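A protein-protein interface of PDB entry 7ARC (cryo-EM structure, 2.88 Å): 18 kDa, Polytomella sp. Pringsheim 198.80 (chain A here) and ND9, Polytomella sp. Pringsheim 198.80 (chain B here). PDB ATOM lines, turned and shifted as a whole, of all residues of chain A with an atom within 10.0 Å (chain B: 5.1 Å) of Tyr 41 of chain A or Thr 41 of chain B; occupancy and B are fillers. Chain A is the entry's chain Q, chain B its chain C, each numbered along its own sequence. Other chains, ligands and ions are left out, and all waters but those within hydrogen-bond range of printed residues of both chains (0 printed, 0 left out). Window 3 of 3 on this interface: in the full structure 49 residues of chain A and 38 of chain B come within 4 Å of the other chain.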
ATOM      1  N   ALA A  33     -16.669 -18.338  17.542  1.00  0.00           N
ATOM      2  CA  ALA A  33     -17.276 -18.978  18.701  1.00  0.00           C
ATOM      3  C   ALA A  33     -17.798 -20.364  18.362  1.00  0.00           C
ATOM      4  O   ALA A  33     -17.790 -21.251  19.221  1.00  0.00           O
ATOM      5  CB  ALA A  33     -18.400 -18.106  19.255  1.00  0.00           C
ATOM      6  N   MET A  34     -18.236 -20.577  17.120  1.00  0.00           N
ATOM      7  CA  MET A  34     -18.674 -21.908  16.707  1.00  0.00           C
ATOM      8  C   MET A  34     -17.533 -22.916  16.809  1.00  0.00           C
ATOM      9  O   MET A  34     -17.667 -23.972  17.443  1.00  0.00           O
ATOM     10  CB  MET A  34     -19.223 -21.850  15.283  1.00  0.00           C
ATOM     11  CG  MET A  34     -20.490 -21.021  15.139  1.00  0.00           C
ATOM     12  SD  MET A  34     -21.881 -21.631  16.106  1.00  0.00           S
ATOM     13  CE  MET A  34     -22.258 -23.146  15.230  1.00  0.00           C
ATOM     14  N   LYS A  35     -16.393 -22.600  16.190  1.00  0.00           N
ATOM     15  CA  LYS A  35     -15.234 -23.483  16.258  1.00  0.00           C
ATOM     16  C   LYS A  35     -14.740 -23.645  17.690  1.00  0.00           C
ATOM     17  O   LYS A  35     -14.270 -24.724  18.076  1.00  0.00           O
ATOM     18  CB  LYS A  35     -14.109 -22.941  15.375  1.00  0.00           C
ATOM     19  CG  LYS A  35     -14.422 -22.796  13.883  1.00  0.00           C
ATOM     20  CD  LYS A  35     -14.546 -24.126  13.147  1.00  0.00           C
ATOM     21  CE  LYS A  35     -15.987 -24.610  13.071  1.00  0.00           C
ATOM     22  NZ  LYS A  35     -16.111 -25.851  12.260  1.00  0.00           N
ATOM     23  N   LYS A  36     -14.818 -22.580  18.492  1.00  0.00           N
ATOM     24  CA  LYS A  36     -14.302 -22.669  19.853  1.00  0.00           C
ATOM     25  C   LYS A  36     -15.186 -23.585  20.696  1.00  0.00           C
ATOM     26  O   LYS A  36     -14.686 -24.391  21.491  1.00  0.00           O
ATOM     27  CB  LYS A  36     -14.216 -21.267  20.454  1.00  0.00           C
ATOM     28  CG  LYS A  36     -13.648 -21.170  21.857  1.00  0.00           C
ATOM     29  CD  LYS A  36     -12.170 -21.553  21.797  1.00  0.00           C
ATOM     30  CE  LYS A  36     -11.451 -21.418  23.126  1.00  0.00           C
ATOM     31  NZ  LYS A  36     -11.914 -22.361  24.162  1.00  0.00           N
ATOM     32  N   ALA A  37     -16.507 -23.483  20.514  1.00  0.00           N
ATOM     33  CA  ALA A  37     -17.441 -24.420  21.131  1.00  0.00           C
ATOM     34  C   ALA A  37     -17.184 -25.842  20.656  1.00  0.00           C
ATOM     35  O   ALA A  37     -17.359 -26.801  21.416  1.00  0.00           O
ATOM     36  CB  ALA A  37     -18.880 -24.006  20.831  1.00  0.00           C
ATOM     37  N   ASP A  38     -16.786 -25.998  19.393  1.00  0.00           N
ATOM     38  CA  ASP A  38     -16.445 -27.323  18.888  1.00  0.00           C
ATOM     39  C   ASP A  38     -15.254 -27.898  19.641  1.00  0.00           C
ATOM     40  O   ASP A  38     -15.273 -29.057  20.068  1.00  0.00           O
ATOM     41  CB  ASP A  38     -16.146 -27.263  17.389  1.00  0.00           C
ATOM     42  CG  ASP A  38     -17.373 -26.968  16.567  1.00  0.00           C
ATOM     43  OD1 ASP A  38     -18.475 -27.336  17.011  1.00  0.00           O
ATOM     44  OD2 ASP A  38     -17.240 -26.380  15.475  1.00  0.00           O
ATOM     45  N   GLU A  39     -14.199 -27.100  19.804  1.00  0.00           N
ATOM     46  CA  GLU A  39     -12.974 -27.642  20.379  1.00  0.00           C
ATOM     47  C   GLU A  39     -13.076 -27.826  21.891  1.00  0.00           C
ATOM     48  O   GLU A  39     -12.404 -28.705  22.442  1.00  0.00           O
ATOM     49  CB  GLU A  39     -11.772 -26.763  20.026  1.00  0.00           C
ATOM     50  CG  GLU A  39     -11.889 -25.308  20.413  1.00  0.00           C
ATOM     51  CD  GLU A  39     -10.820 -24.454  19.756  1.00  0.00           C
ATOM     52  OE1 GLU A  39     -11.135 -23.327  19.321  1.00  0.00           O
ATOM     53  OE2 GLU A  39      -9.663 -24.917  19.667  1.00  0.00           O
ATOM     54  N   ILE A  40     -13.896 -27.026  22.579  1.00  0.00           N
ATOM     55  CA  ILE A  40     -14.055 -27.221  24.021  1.00  0.00           C
ATOM     56  C   ILE A  40     -14.778 -28.527  24.320  1.00  0.00           C
ATOM     57  O   ILE A  40     -14.394 -29.269  25.234  1.00  0.00           O
ATOM     58  CB  ILE A  40     -14.788 -26.032  24.669  1.00  0.00           C
ATOM     59  CG1 ILE A  40     -13.981 -24.749  24.531  1.00  0.00           C
ATOM     60  CG2 ILE A  40     -15.084 -26.315  26.133  1.00  0.00           C
ATOM     61  CD1 ILE A  40     -14.759 -23.526  24.926  1.00  0.00           C
ATOM     62  N   TYR A  41     -15.820 -28.839  23.561  1.00  0.00           N
ATOM     63  CA  TYR A  41     -16.687 -29.965  23.865  1.00  0.00           C
ATOM     64  C   TYR A  41     -16.342 -31.176  23.006  1.00  0.00           C
ATOM     65  O   TYR A  41     -15.617 -31.089  22.013  1.00  0.00           O
ATOM     66  CB  TYR A  41     -18.152 -29.569  23.662  1.00  0.00           C
ATOM     67  CG  TYR A  41     -18.693 -28.689  24.761  1.00  0.00           C
ATOM     68  CD1 TYR A  41     -18.949 -29.201  26.024  1.00  0.00           C
ATOM     69  CD2 TYR A  41     -18.935 -27.340  24.540  1.00  0.00           C
ATOM     70  CE1 TYR A  41     -19.440 -28.400  27.031  1.00  0.00           C
ATOM     71  CE2 TYR A  41     -19.427 -26.530  25.542  1.00  0.00           C
ATOM     72  CZ  TYR A  41     -19.676 -27.065  26.785  1.00  0.00           C
ATOM     73  OH  TYR A  41     -20.165 -26.264  27.788  1.00  0.00           O
ATOM     74  N   SER A  42     -16.877 -32.323  23.411  1.00  0.00           N
ATOM     75  CA  SER A  42     -16.604 -33.584  22.738  1.00  0.00           C
ATOM     76  C   SER A  42     -17.747 -34.547  23.019  1.00  0.00           C
ATOM     77  O   SER A  42     -18.565 -34.331  23.917  1.00  0.00           O
ATOM     78  CB  SER A  42     -15.266 -34.179  23.186  1.00  0.00           C
ATOM     79  OG  SER A  42     -15.024 -35.422  22.551  1.00  0.00           O
ATOM     80  N   GLY A  43     -17.792 -35.617  22.234  1.00  0.00           N
ATOM     81  CA  GLY A  43     -18.828 -36.627  22.339  1.00  0.00           C
ATOM     82  C   GLY A  43     -18.261 -37.923  22.885  1.00  0.00           C
ATOM     83  O   GLY A  43     -17.115 -38.280  22.608  1.00  0.00           O
ATOM     84  N   LYS A  44     -19.074 -38.626  23.668  1.00  0.00           N
ATOM     85  CA  LYS A  44     -18.661 -39.899  24.238  1.00  0.00           C
ATOM     86  C   LYS A  44     -18.710 -40.994  23.181  1.00  0.00           C
ATOM     87  O   LYS A  44     -19.634 -41.050  22.365  1.00  0.00           O
ATOM     88  CB  LYS A  44     -19.566 -40.273  25.412  1.00  0.00           C
ATOM     89  CG  LYS A  44     -19.536 -39.290  26.568  1.00  0.00           C
ATOM     90  CD  LYS A  44     -18.148 -39.199  27.178  1.00  0.00           C
ATOM     91  CE  LYS A  44     -17.762 -40.504  27.854  1.00  0.00           C
ATOM     92  NZ  LYS A  44     -18.636 -40.811  29.021  1.00  0.00           N
ATOM     93  N   TYR B  39     -18.441 -23.155  36.849  1.00  0.00           N
ATOM     94  CA  TYR B  39     -19.576 -23.473  35.988  1.00  0.00           C
ATOM     95  C   TYR B  39     -19.336 -23.027  34.551  1.00  0.00           C
ATOM     96  O   TYR B  39     -19.710 -23.731  33.607  1.00  0.00           O
ATOM     97  CB  TYR B  39     -20.852 -22.841  36.541  1.00  0.00           C
ATOM     98  CG  TYR B  39     -21.171 -23.216  37.972  1.00  0.00           C
ATOM     99  CD1 TYR B  39     -20.653 -24.369  38.543  1.00  0.00           C
ATOM    100  CD2 TYR B  39     -21.998 -22.418  38.747  1.00  0.00           C
ATOM    101  CE1 TYR B  39     -20.946 -24.713  39.842  1.00  0.00           C
ATOM    102  CE2 TYR B  39     -22.296 -22.755  40.048  1.00  0.00           C
ATOM    103  CZ  TYR B  39     -21.768 -23.903  40.590  1.00  0.00           C
ATOM    104  OH  TYR B  39     -22.064 -24.244  41.888  1.00  0.00           O
ATOM    105  N   VAL B  40     -18.716 -21.870  34.364  1.00  0.00           N
ATOM    106  CA  VAL B  40     -18.595 -21.268  33.042  1.00  0.00           C
ATOM    107  C   VAL B  40     -17.384 -21.847  32.325  1.00  0.00           C
ATOM    108  O   VAL B  40     -16.301 -21.971  32.908  1.00  0.00           O
ATOM    109  CB  VAL B  40     -18.493 -19.739  33.156  1.00  0.00           C
ATOM    110  CG1 VAL B  40     -18.266 -19.115  31.792  1.00  0.00           C
ATOM    111  CG2 VAL B  40     -19.734 -19.176  33.817  1.00  0.00           C
ATOM    112  N   THR B  41     -17.563 -22.205  31.055  1.00  0.00           N
ATOM    113  CA  THR B  41     -16.467 -22.617  30.185  1.00  0.00           C
ATOM    114  C   THR B  41     -16.097 -21.566  29.150  1.00  0.00           C
ATOM    115  O   THR B  41     -14.911 -21.331  28.916  1.00  0.00           O
ATOM    116  CB  THR B  41     -16.813 -23.928  29.471  1.00  0.00           C
ATOM    117  OG1 THR B  41     -17.724 -23.664  28.398  1.00  0.00           O
ATOM    118  CG2 THR B  41     -17.446 -24.909  30.438  1.00  0.00           C
ATOM    119  N   MET B  42     -17.083 -20.932  28.522  1.00  0.00           N
ATOM    120  CA  MET B  42     -16.848 -19.801  27.638  1.00  0.00           C
ATOM    121  C   MET B  42     -18.081 -18.913  27.646  1.00  0.00           C
ATOM    122  O   MET B  42     -19.172 -19.337  28.034  1.00  0.00           O
ATOM    123  CB  MET B  42     -16.522 -20.235  26.205  1.00  0.00           C
ATOM    124  CG  MET B  42     -17.660 -20.941  25.502  1.00  0.00           C
ATOM    125  SD  MET B  42     -17.275 -21.429  23.812  1.00  0.00           S
ATOM    126  CE  MET B  42     -17.281 -19.835  23.000  1.00  0.00           C
ATOM    127  N   ALA B  43     -17.894 -17.670  27.220  1.00  0.00           N
ATOM    128  CA  ALA B  43     -18.959 -16.680  27.184  1.00  0.00           C
ATOM    129  C   ALA B  43     -18.927 -15.946  25.854  1.00  0.00           C
ATOM    130  O   ALA B  43     -17.854 -15.692  25.305  1.00  0.00           O
ATOM    131  CB  ALA B  43     -18.827 -15.691  28.333  1.00  0.00           C
ATOM    132  N   TYR B  60     -21.759 -20.702  28.068  1.00  0.00           N
ATOM    133  CA  TYR B  60     -21.674 -22.127  27.782  1.00  0.00           C
ATOM    134  C   TYR B  60     -21.232 -22.831  29.054  1.00  0.00           C
ATOM    135  O   TYR B  60     -20.200 -22.485  29.634  1.00  0.00           O
ATOM    136  CB  TYR B  60     -20.689 -22.414  26.651  1.00  0.00           C
ATOM    137  CG  TYR B  60     -21.112 -21.915  25.293  1.00  0.00           C
ATOM    138  CD1 TYR B  60     -21.111 -20.561  24.997  1.00  0.00           C
ATOM    139  CD2 TYR B  60     -21.496 -22.800  24.301  1.00  0.00           C
ATOM    140  CE1 TYR B  60     -21.488 -20.106  23.755  1.00  0.00           C
ATOM    141  CE2 TYR B  60     -21.875 -22.353  23.056  1.00  0.00           C
ATOM    142  CZ  TYR B  60     -21.870 -21.006  22.788  1.00  0.00           C
ATOM    143  OH  TYR B  60     -22.249 -20.557  21.547  1.00  0.00           O
ATOM    144  N   THR B  61     -22.015 -23.812  29.487  1.00  0.00           N
ATOM    145  CA  THR B  61     -21.693 -24.592  30.668  1.00  0.00           C
ATOM    146  C   THR B  61     -21.923 -26.064  30.363  1.00  0.00           C
ATOM    147  O   THR B  61     -22.561 -26.422  29.373  1.00  0.00           O
ATOM    148  CB  THR B  61     -22.525 -24.151  31.880  1.00  0.00           C
ATOM    149  OG1 THR B  61     -22.075 -24.839  33.053  1.00  0.00           O
ATOM    150  CG2 THR B  61     -23.988 -24.452  31.658  1.00  0.00           C
ATOM    151  N   THR B  62     -21.375 -26.907  31.206  1.00  0.00           N
ATOM    152  CA  THR B  62     -21.453 -28.345  31.033  1.00  0.00           C
ATOM    153  C   THR B  62     -22.698 -28.902  31.713  1.00  0.00           C
ATOM    154  O   THR B  62     -23.259 -28.270  32.612  1.00  0.00           O
ATOM    155  CB  THR B  62     -20.196 -28.999  31.600  1.00  0.00           C
ATOM    156  OG1 THR B  62     -20.105 -28.715  33.001  1.00  0.00           O
ATOM    157  CG2 THR B  62     -18.962 -28.464  30.900  1.00  0.00           C
ATOM    158  N   ALA B  97     -20.545 -33.780  19.665  1.00  0.00           N
ATOM    159  CA  ALA B  97     -21.610 -33.448  20.612  1.00  0.00           C
ATOM    160  C   ALA B  97     -22.686 -32.685  19.849  1.00  0.00           C
ATOM    161  O   ALA B  97     -22.633 -31.464  19.709  1.00  0.00           O
ATOM    162  CB  ALA B  97     -21.059 -32.649  21.783  1.00  0.00           C
ATOM    163  N   LYS B 117     -26.193 -22.264  27.409  1.00  0.00           N
ATOM    164  CA  LYS B 117     -26.087 -23.378  26.476  1.00  0.00           C
ATOM    165  C   LYS B 117     -25.342 -24.534  27.126  1.00  0.00           C
ATOM    166  O   LYS B 117     -24.279 -24.338  27.720  1.00  0.00           O
ATOM    167  CB  LYS B 117     -25.386 -22.976  25.182  1.00  0.00           C
ATOM    168  CG  LYS B 117     -26.167 -22.015  24.326  1.00  0.00           C
ATOM    169  CD  LYS B 117     -25.406 -21.710  23.059  1.00  0.00           C
ATOM    170  CE  LYS B 117     -26.152 -20.732  22.187  1.00  0.00           C
ATOM    171  NZ  LYS B 117     -25.381 -20.441  20.954  1.00  0.00           N
ATOM    172  N   VAL B 119     -23.893 -28.236  25.879  1.00  0.00           N
ATOM    173  CA  VAL B 119     -23.604 -29.022  24.685  1.00  0.00           C
ATOM    174  C   VAL B 119     -23.473 -30.484  25.091  1.00  0.00           C
ATOM    175  O   VAL B 119     -22.593 -30.839  25.883  1.00  0.00           O
ATOM    176  CB  VAL B 119     -22.333 -28.523  23.983  1.00  0.00           C
ATOM    177  CG1 VAL B 119     -22.003 -29.409  22.812  1.00  0.00           C
ATOM    178  CG2 VAL B 119     -22.508 -27.085  23.528  1.00  0.00           C
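The side-chain hydroxyl (OH) of Tyr 41 of chain A is in hydrogen-bond range of the backbone carbonyl oxygen (O) of Thr 61 of chain B.
The side-chain hydroxyl of Thr 61 of chain B lies within hydrogen-bond range of the backbone carbonyl oxygen of Tyr 39 of chain B (2.7 Å). The side-chain hydroxyl (OG1) of Thr 41 of chain B sits at hydrogen-bond distance from the backbone carbonyl oxygen (O) of Tyr 60 of chain B (3.0 Å). The backbone NH of Tyr 60 of chain B sits at hydrogen-bond distance from the backbone carbonyl oxygen of Met 42 of chain B, 2.9 Å away. NZ of Lys 117 of chain B lies within hydrogen-bond range of OH of Tyr 60 of chain B (3.2 Å). N of Thr 61 of chain B is in hydrogen-bond range of O of Lys 117 of chain B, at 2.9 Å.
Met 42 of chain B touches Ala 37 of chain A (SD to N, 3.96 Å). CD1 of Ile 40 of chain A touches SD of Met 42 of chain B, 3.5 Å away. Tyr 41 of chain A touches Thr 41 of chain B. Tyr 60 of chain B touches Tyr 41 of chain A (C to OH, 3.8 Å). N of Thr 62 of chain B touches OH of Tyr 41 of chain A (3.7 Å). Tyr 41 of chain A touches Val 119 of chain B. Ala 97 of chain B touches Ser 42 of chain A (CB to O, 3.7 Å).
Lys 35 of chain A touches none of the printed residues of chain B. Of chain A, only Tyr 41 (3.6 Å) comes within 4 Å of Thr 41 of chain B. Printed residues of chain A within 4 Å of Met 42 of chain B: Ala 37 (3.96 Å) and Ile 40 (3.5 Å). Of the printed residues of chain A, Tyr 60 of chain B touches Tyr 41. Of chain A, only Tyr 41 (2.9 Å) comes within 4 Å of Thr 61 of chain B. Printed residues of chain A within 4 Å of Ala 97 of chain B: Ser 42 (3.7 Å). Val 119 of chain B touches just one residue of chain A: Tyr 41 (3.6 Å). The nearest printed residue of chain A that does not touch Tyr 60 of chain B is Ala 37 of chain A (4.1 Å).
Of the 11 printed residues of chain B, 7 touch a printed residue of chain A. Hydrophobic or aromatic side chains of chain B within 4 Å of the printed part of chain A: Met 42, Ala 97 and Val 119. Along chain B the printed residues that touch a printed residue of chain A span positions 41 to 119. Among the printed residues, 8 pairs touch across the chains. Among the printed residues, no Asp or Glu carboxylate lies within 4 Å of a Lys or Arg side-chain nitrogen of the other chain.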
